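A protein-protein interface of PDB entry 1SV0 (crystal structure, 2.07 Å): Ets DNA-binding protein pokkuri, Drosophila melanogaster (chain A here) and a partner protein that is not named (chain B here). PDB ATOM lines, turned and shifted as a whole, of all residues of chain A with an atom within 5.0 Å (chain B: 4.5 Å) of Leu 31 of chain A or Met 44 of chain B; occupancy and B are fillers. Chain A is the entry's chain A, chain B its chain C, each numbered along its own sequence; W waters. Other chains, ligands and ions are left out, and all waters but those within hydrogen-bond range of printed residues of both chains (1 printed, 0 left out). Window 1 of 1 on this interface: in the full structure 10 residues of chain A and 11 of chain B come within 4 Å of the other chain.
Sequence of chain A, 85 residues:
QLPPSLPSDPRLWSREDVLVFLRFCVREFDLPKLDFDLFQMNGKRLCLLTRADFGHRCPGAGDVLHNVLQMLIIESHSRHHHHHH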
ATOM      1  N   CYS A  25     -26.334 -15.826  21.588  1.00  0.00           N
ATOM      2  CA  CYS A  25     -27.265 -15.820  20.451  1.00  0.00           C
ATOM      3  C   CYS A  25     -26.562 -15.997  19.107  1.00  0.00           C
ATOM      4  O   CYS A  25     -27.054 -16.705  18.238  1.00  0.00           O
ATOM      5  CB  CYS A  25     -28.073 -14.525  20.417  1.00  0.00           C
ATOM      6  SG  CYS A  25     -29.356 -14.439  21.686  1.00  0.00           S
ATOM      7  N   VAL A  26     -25.422 -15.336  18.937  1.00  0.00           N
ATOM      8  CA  VAL A  26     -24.662 -15.438  17.704  1.00  0.00           C
ATOM      9  C   VAL A  26     -24.285 -16.902  17.461  1.00  0.00           C
ATOM     10  O   VAL A  26     -24.384 -17.392  16.341  1.00  0.00           O
ATOM     11  CB  VAL A  26     -23.403 -14.558  17.775  1.00  0.00           C
ATOM     12  CG1 VAL A  26     -22.330 -15.064  16.797  1.00  0.00           C
ATOM     13  CG2 VAL A  26     -23.787 -13.118  17.436  1.00  0.00           C
ATOM     14  N   PHE A  29     -27.709 -19.289  17.095  1.00  0.00           N
ATOM     15  CA  PHE A  29     -28.436 -19.103  15.852  1.00  0.00           C
ATOM     16  C   PHE A  29     -27.529 -19.051  14.623  1.00  0.00           C
ATOM     17  O   PHE A  29     -28.008 -18.873  13.517  1.00  0.00           O
ATOM     18  CB  PHE A  29     -29.284 -17.834  15.961  1.00  0.00           C
ATOM     19  CG  PHE A  29     -30.324 -17.905  17.039  1.00  0.00           C
ATOM     20  CD1 PHE A  29     -30.456 -16.883  17.969  1.00  0.00           C
ATOM     21  CD2 PHE A  29     -31.166 -19.011  17.136  1.00  0.00           C
ATOM     22  CE1 PHE A  29     -31.408 -16.957  18.974  1.00  0.00           C
ATOM     23  CE2 PHE A  29     -32.122 -19.094  18.140  1.00  0.00           C
ATOM     24  CZ  PHE A  29     -32.243 -18.067  19.064  1.00  0.00           C
ATOM     25  N   ASP A  30     -26.224 -19.216  14.829  1.00  0.00           N
ATOM     26  CA  ASP A  30     -25.253 -19.202  13.731  1.00  0.00           C
ATOM     27  C   ASP A  30     -25.358 -17.886  12.955  1.00  0.00           C
ATOM     28  O   ASP A  30     -25.450 -17.876  11.723  1.00  0.00           O
ATOM     29  CB  ASP A  30     -25.507 -20.389  12.784  1.00  0.00           C
ATOM     30  CG  ASP A  30     -24.272 -20.779  11.968  1.00  0.00           C
ATOM     31  OD1 ASP A  30     -23.272 -20.034  11.987  1.00  0.00           O
ATOM     32  OD2 ASP A  30     -24.303 -21.840  11.298  1.00  0.00           O
ATOM     33  N   LEU A  31     -25.347 -16.777  13.688  1.00  0.00           N
ATOM     34  CA  LEU A  31     -25.435 -15.450  13.082  1.00  0.00           C
ATOM     35  C   LEU A  31     -24.063 -14.945  12.640  1.00  0.00           C
ATOM     36  O   LEU A  31     -23.034 -15.414  13.116  1.00  0.00           O
ATOM     37  CB  LEU A  31     -26.021 -14.462  14.085  1.00  0.00           C
ATOM     38  CG  LEU A  31     -27.354 -14.852  14.725  1.00  0.00           C
ATOM     39  CD1 LEU A  31     -27.760 -13.756  15.697  1.00  0.00           C
ATOM     40  CD2 LEU A  31     -28.425 -15.058  13.656  1.00  0.00           C
ATOM     41  N   PRO A  32     -24.029 -13.975  11.714  1.00  0.00           N
ATOM     42  CA  PRO A  32     -22.719 -13.478  11.287  1.00  0.00           C
ATOM     43  C   PRO A  32     -22.136 -12.607  12.401  1.00  0.00           C
ATOM     44  O   PRO A  32     -22.854 -12.200  13.313  1.00  0.00           O
ATOM     45  CB  PRO A  32     -23.051 -12.691  10.024  1.00  0.00           C
ATOM     46  CG  PRO A  32     -24.395 -12.107  10.357  1.00  0.00           C
ATOM     47  CD  PRO A  32     -25.121 -13.272  11.015  1.00  0.00           C
ATOM     48  N   LYS A  33     -20.838 -12.337  12.331  1.00  0.00           N
ATOM     49  CA  LYS A  33     -20.172 -11.523  13.343  1.00  0.00           C
ATOM     50  C   LYS A  33     -21.015 -10.310  13.697  1.00  0.00           C
ATOM     51  O   LYS A  33     -21.453  -9.569  12.824  1.00  0.00           O
ATOM     52  CB  LYS A  33     -18.801 -11.078  12.832  1.00  0.00           C
ATOM     53  CG  LYS A  33     -17.905 -12.240  12.403  1.00  0.00           C
ATOM     54  CD  LYS A  33     -16.520 -11.768  11.976  1.00  0.00           C
ATOM     55  CE  LYS A  33     -15.642 -12.943  11.555  1.00  0.00           C
ATOM     56  NZ  LYS A  33     -14.295 -12.497  11.090  1.00  0.00           N
ATOM     57  N   CYS A  58     -28.305  -5.277  13.575  1.00  0.00           N
ATOM     58  CA  CYS A  58     -28.059  -6.645  13.138  1.00  0.00           C
ATOM     59  C   CYS A  58     -28.907  -6.916  11.909  1.00  0.00           C
ATOM     60  O   CYS A  58     -29.963  -7.540  11.996  1.00  0.00           O
ATOM     61  CB  CYS A  58     -28.423  -7.644  14.241  1.00  0.00           C
ATOM     62  SG  CYS A  58     -28.152  -9.379  13.781  1.00  0.00           S
ATOM     63  N   GLY A  60     -30.480  -8.589   8.837  1.00  0.00           N
ATOM     64  CA  GLY A  60     -30.643  -9.988   8.502  1.00  0.00           C
ATOM     65  C   GLY A  60     -31.205 -10.838   9.627  1.00  0.00           C
ATOM     66  O   GLY A  60     -31.892 -11.818   9.359  1.00  0.00           O
ATOM     67  N   ALA A  61     -30.931 -10.476  10.879  1.00  0.00           N
ATOM     68  CA  ALA A  61     -31.433 -11.262  12.008  1.00  0.00           C
ATOM     69  C   ALA A  61     -31.884 -10.445  13.219  1.00  0.00           C
ATOM     70  O   ALA A  61     -32.219 -11.012  14.258  1.00  0.00           O
ATOM     71  CB  ALA A  61     -30.376 -12.273  12.445  1.00  0.00           C
ATOM     72  N   VAL A  64     -35.258 -11.449  14.717  1.00  0.00           N
ATOM     73  CA  VAL A  64     -35.233 -12.694  15.476  1.00  0.00           C
ATOM     74  C   VAL A  64     -34.734 -12.396  16.896  1.00  0.00           C
ATOM     75  O   VAL A  64     -35.368 -12.778  17.878  1.00  0.00           O
ATOM     76  CB  VAL A  64     -34.284 -13.735  14.839  1.00  0.00           C
ATOM     77  CG1 VAL A  64     -34.133 -14.942  15.770  1.00  0.00           C
ATOM     78  CG2 VAL A  64     -34.828 -14.171  13.488  1.00  0.00           C
ATOM     79  N   LEU A  65     -33.598 -11.712  16.995  1.00  0.00           N
ATOM     80  CA  LEU A  65     -33.023 -11.369  18.301  1.00  0.00           C
ATOM     81  C   LEU A  65     -34.022 -10.604  19.152  1.00  0.00           C
ATOM     82  O   LEU A  65     -34.181 -10.880  20.341  1.00  0.00           O
ATOM     83  CB  LEU A  65     -31.761 -10.514  18.134  1.00  0.00           C
ATOM     84  CG  LEU A  65     -30.569 -11.178  17.452  1.00  0.00           C
ATOM     85  CD1 LEU A  65     -29.432 -10.169  17.335  1.00  0.00           C
ATOM     86  CD2 LEU A  65     -30.131 -12.403  18.265  1.00  0.00           C
ATOM     87  N   THR B  15     -27.541 -25.940  10.105  1.00  0.00           N
ATOM     88  CA  THR B  15     -26.610 -24.844  10.379  1.00  0.00           C
ATOM     89  C   THR B  15     -27.022 -23.751   9.395  1.00  0.00           C
ATOM     90  O   THR B  15     -27.998 -23.912   8.664  1.00  0.00           O
ATOM     91  CB  THR B  15     -25.171 -25.234  10.055  1.00  0.00           C
ATOM     92  OG1 THR B  15     -25.100 -25.606   8.672  1.00  0.00           O
ATOM     93  CG2 THR B  15     -24.714 -26.413  10.938  1.00  0.00           C
ATOM     94  N   ARG B  16     -26.291 -22.644   9.365  1.00  0.00           N
ATOM     95  CA  ARG B  16     -26.632 -21.581   8.428  1.00  0.00           C
ATOM     96  C   ARG B  16     -26.386 -22.112   7.022  1.00  0.00           C
ATOM     97  O   ARG B  16     -27.168 -21.852   6.102  1.00  0.00           O
ATOM     98  CB  ARG B  16     -25.774 -20.337   8.684  1.00  0.00           C
ATOM     99  CG  ARG B  16     -26.092 -19.172   7.758  1.00  0.00           C
ATOM    100  CD  ARG B  16     -25.446 -17.899   8.267  1.00  0.00           C
ATOM    101  NE  ARG B  16     -24.006 -17.910   8.082  1.00  0.00           N
ATOM    102  CZ  ARG B  16     -23.174 -17.079   8.694  1.00  0.00           C
ATOM    103  NH1 ARG B  16     -23.644 -16.169   9.541  1.00  0.00           N
ATOM    104  NH2 ARG B  16     -21.874 -17.158   8.456  1.00  0.00           N
ATOM    105  N   VAL B  19     -29.322 -24.026   5.869  1.00  0.00           N
ATOM    106  CA  VAL B  19     -30.401 -23.096   5.553  1.00  0.00           C
ATOM    107  C   VAL B  19     -30.231 -22.526   4.134  1.00  0.00           C
ATOM    108  O   VAL B  19     -31.186 -22.464   3.354  1.00  0.00           O
ATOM    109  CB  VAL B  19     -30.435 -21.924   6.556  1.00  0.00           C
ATOM    110  CG1 VAL B  19     -31.368 -20.829   6.047  1.00  0.00           C
ATOM    111  CG2 VAL B  19     -30.901 -22.426   7.922  1.00  0.00           C
ATOM    112  N   PHE B  42     -31.193 -14.416   4.994  1.00  0.00           N
ATOM    113  CA  PHE B  42     -31.319 -15.400   6.064  1.00  0.00           C
ATOM    114  C   PHE B  42     -29.972 -15.854   6.622  1.00  0.00           C
ATOM    115  O   PHE B  42     -29.584 -17.011   6.455  1.00  0.00           O
ATOM    116  CB  PHE B  42     -32.078 -16.643   5.573  1.00  0.00           C
ATOM    117  CG  PHE B  42     -33.457 -16.358   5.051  1.00  0.00           C
ATOM    118  CD1 PHE B  42     -33.644 -15.875   3.762  1.00  0.00           C
ATOM    119  CD2 PHE B  42     -34.579 -16.602   5.841  1.00  0.00           C
ATOM    120  CE1 PHE B  42     -34.926 -15.648   3.263  1.00  0.00           C
ATOM    121  CE2 PHE B  42     -35.864 -16.378   5.354  1.00  0.00           C
ATOM    122  CZ  PHE B  42     -36.036 -15.898   4.058  1.00  0.00           C
ATOM    123  N   PRO B  43     -29.234 -14.949   7.278  1.00  0.00           N
ATOM    124  CA  PRO B  43     -27.934 -15.308   7.847  1.00  0.00           C
ATOM    125  C   PRO B  43     -28.147 -15.961   9.224  1.00  0.00           C
ATOM    126  O   PRO B  43     -27.746 -15.400  10.245  1.00  0.00           O
ATOM    127  CB  PRO B  43     -27.233 -13.954   7.953  1.00  0.00           C
ATOM    128  CG  PRO B  43     -28.362 -13.050   8.345  1.00  0.00           C
ATOM    129  CD  PRO B  43     -29.493 -13.502   7.422  1.00  0.00           C
ATOM    130  N   MET B  44     -28.770 -17.139   9.245  1.00  0.00           N
ATOM    131  CA  MET B  44     -29.068 -17.834  10.499  1.00  0.00           C
ATOM    132  C   MET B  44     -29.244 -19.337  10.269  1.00  0.00           C
ATOM    133  O   MET B  44     -29.317 -19.782   9.122  1.00  0.00           O
ATOM    134  CB  MET B  44     -30.356 -17.260  11.087  1.00  0.00           C
ATOM    135  CG  MET B  44     -31.536 -17.382  10.120  1.00  0.00           C
ATOM    136  SD  MET B  44     -33.061 -16.558  10.644  1.00  0.00           S
ATOM    137  CE  MET B  44     -32.714 -14.880  10.112  1.00  0.00           C
ATOM    138  N   ASN B  45     -29.340 -20.109  11.353  1.00  0.00           N
ATOM    139  CA  ASN B  45     -29.505 -21.562  11.249  1.00  0.00           C
ATOM    140  C   ASN B  45     -30.957 -22.014  11.425  1.00  0.00           C
ATOM    141  O   ASN B  45     -31.868 -21.190  11.521  1.00  0.00           O
ATOM    142  CB  ASN B  45     -28.604 -22.291  12.266  1.00  0.00           C
ATOM    143  CG  ASN B  45     -29.002 -22.031  13.720  1.00  0.00           C
ATOM    144  OD1 ASN B  45     -30.051 -21.460  14.003  1.00  0.00           O
ATOM    145  ND2 ASN B  45     -28.157 -22.469  14.647  1.00  0.00           N
ATOM    146  N   ALA B  48     -33.056 -20.734  14.477  1.00  0.00           N
ATOM    147  CA  ALA B  48     -33.577 -19.389  14.268  1.00  0.00           C
ATOM    148  C   ALA B  48     -34.826 -19.423  13.397  1.00  0.00           C
ATOM    149  O   ALA B  48     -35.795 -18.704  13.662  1.00  0.00           O
ATOM    150  CB  ALA B  48     -32.504 -18.494  13.614  1.00  0.00           C
ATOM    151  N   LEU B  49     -34.804 -20.262  12.361  1.00  0.00           N
ATOM    152  CA  LEU B  49     -35.943 -20.372  11.448  1.00  0.00           C
ATOM    153  C   LEU B  49     -37.207 -20.834  12.175  1.00  0.00           C
ATOM    154  O   LEU B  49     -38.311 -20.393  11.853  1.00  0.00           O
ATOM    155  CB  LEU B  49     -35.601 -21.325  10.285  1.00  0.00           C
ATOM    156  CG  LEU B  49     -35.556 -20.720   8.873  1.00  0.00           C
ATOM    157  CD1 LEU B  49     -34.793 -19.407   8.870  1.00  0.00           C
ATOM    158  CD2 LEU B  49     -34.913 -21.718   7.910  1.00  0.00           C
ATOM    159  N   MET B  52     -39.104 -18.012  13.377  1.00  0.00           N
ATOM    160  CA  MET B  52     -39.661 -17.088  12.389  1.00  0.00           C
ATOM    161  C   MET B  52     -41.128 -17.291  12.032  1.00  0.00           C
ATOM    162  O   MET B  52     -41.556 -18.388  11.668  1.00  0.00           O
ATOM    163  CB  MET B  52     -38.842 -17.107  11.095  1.00  0.00           C
ATOM    164  CG  MET B  52     -37.413 -16.601  11.226  1.00  0.00           C
ATOM    165  SD  MET B  52     -36.864 -15.746   9.719  1.00  0.00           S
ATOM    166  CE  MET B  52     -37.294 -16.926   8.480  1.00  0.00           C
ATOM    167  N   ARG B  60     -38.791 -10.650   4.106  1.00  0.00           N
ATOM    168  CA  ARG B  60     -37.537 -10.873   3.409  1.00  0.00           C
ATOM    169  C   ARG B  60     -37.790 -11.249   1.950  1.00  0.00           C
ATOM    170  O   ARG B  60     -37.112 -10.775   1.048  1.00  0.00           O
ATOM    171  CB  ARG B  60     -36.761 -11.984   4.131  1.00  0.00           C
ATOM    172  CG  ARG B  60     -36.884 -11.891   5.658  1.00  0.00           C
ATOM    173  CD  ARG B  60     -36.281 -13.097   6.375  1.00  0.00           C
ATOM    174  NE  ARG B  60     -35.210 -12.707   7.288  1.00  0.00           N
ATOM    175  CZ  ARG B  60     -35.405 -12.095   8.453  1.00  0.00           C
ATOM    176  NH1 ARG B  60     -36.635 -11.809   8.856  1.00  0.00           N
ATOM    177  NH2 ARG B  60     -34.370 -11.748   9.202  1.00  0.00           N
HETATM  178  O   HOH W   1     -23.015 -22.756   8.790  1.00  0.00           O
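The backbone NH (N) of Leu 31 of chain A lies within hydrogen-bond range of the backbone carbonyl oxygen (O) of Val 26 of chain A (2.9 Å).
OD1 of Asn 45 of chain B lies within hydrogen-bond range of N of Ala 48 of chain B.
Among the printed residues, pairs that only touch across the chains: Gly 60 of chain A with Met 44 of chain B (3.3 Å), Leu 31 of chain A with Arg 16 of chain B (3.4 Å), Phe 29 of chain A with Met 44 of chain B (3.4 Å), Pro 32 of chain A with Pro 43 of chain B (3.5 Å), Leu 31 of chain A with Pro 43 of chain B (3.5 Å), Gly 60 of chain A with Pro 43 of chain B (3.5 Å), Asp 30 of chain A with Asn 45 of chain B (3.7 Å), Asp 30 of chain A with Pro 43 of chain B (3.7 Å), Phe 29 of chain A with Ala 48 of chain B (3.7 Å), Asp 30 of chain A with Thr 15 of chain B (3.7 Å), Asp 30 of chain A with Met 44 of chain B (3.8 Å) and Leu 31 of chain A with Met 44 of chain B (3.9 Å).
Water W1 bridges the side-chain carboxylate (OD2) of Asp 30 of chain A (3.0 Å) and the backbone NH (N) of Arg 16 of chain B (3.3 Å).
The backbone carbonyl oxygen (O) of Phe 29 of chain A is in hydrogen-bond range of the backbone NH (N) of Asn 45 of chain B (2.8 Å).
The side-chain carboxylate of Asp 30 of chain A lies within hydrogen-bond range of the backbone NH of Arg 16 of chain B, 2.9 Å away.
O of Gly 60 of chain A lies within hydrogen-bond range of NH2 of Arg 60 of chain B (2.5 Å).
The backbone nitrogen (N) of Pro 32 of chain A sits close to the guanidinium group (NH1) of Arg 16 of chain B, at 3.1 Å.
Leu 31 of chain A touches just these residues of chain B: Arg 16, Pro 43 and Met 44.
Met 44 of chain B touches just these residues of chain A: Phe 29, Asp 30, Leu 31 and Gly 60.
Of the printed residues of chain A, Arg 60 of chain B touches Gly 60.
Printed residues of chain B within 4 Å of Gly 60 of chain A: Pro 43 (3.5 Å), Met 44 (3.3 Å) and Arg 60 (2.5 Å).
Cys 58 of chain A touches none of the printed residues of chain B.
The nearest printed residue of chain B that does not touch Leu 31 of chain A is Ala 48 of chain B (5.3 Å).
The nearest residue of chain A that does not touch Met 44 of chain B is Val 64 of chain A (4.05 Å).
Hydrophobic or aromatic side chains of chain A that line the printed part of chain B: Phe 29, Leu 31 and Pro 32.
Hydrophobic or aromatic side chains of chain B that line the printed part of chain A: Pro 43, Met 44 and Ala 48.
Along chain B the printed residues that touch a printed residue of chain A span positions 15 to 60.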
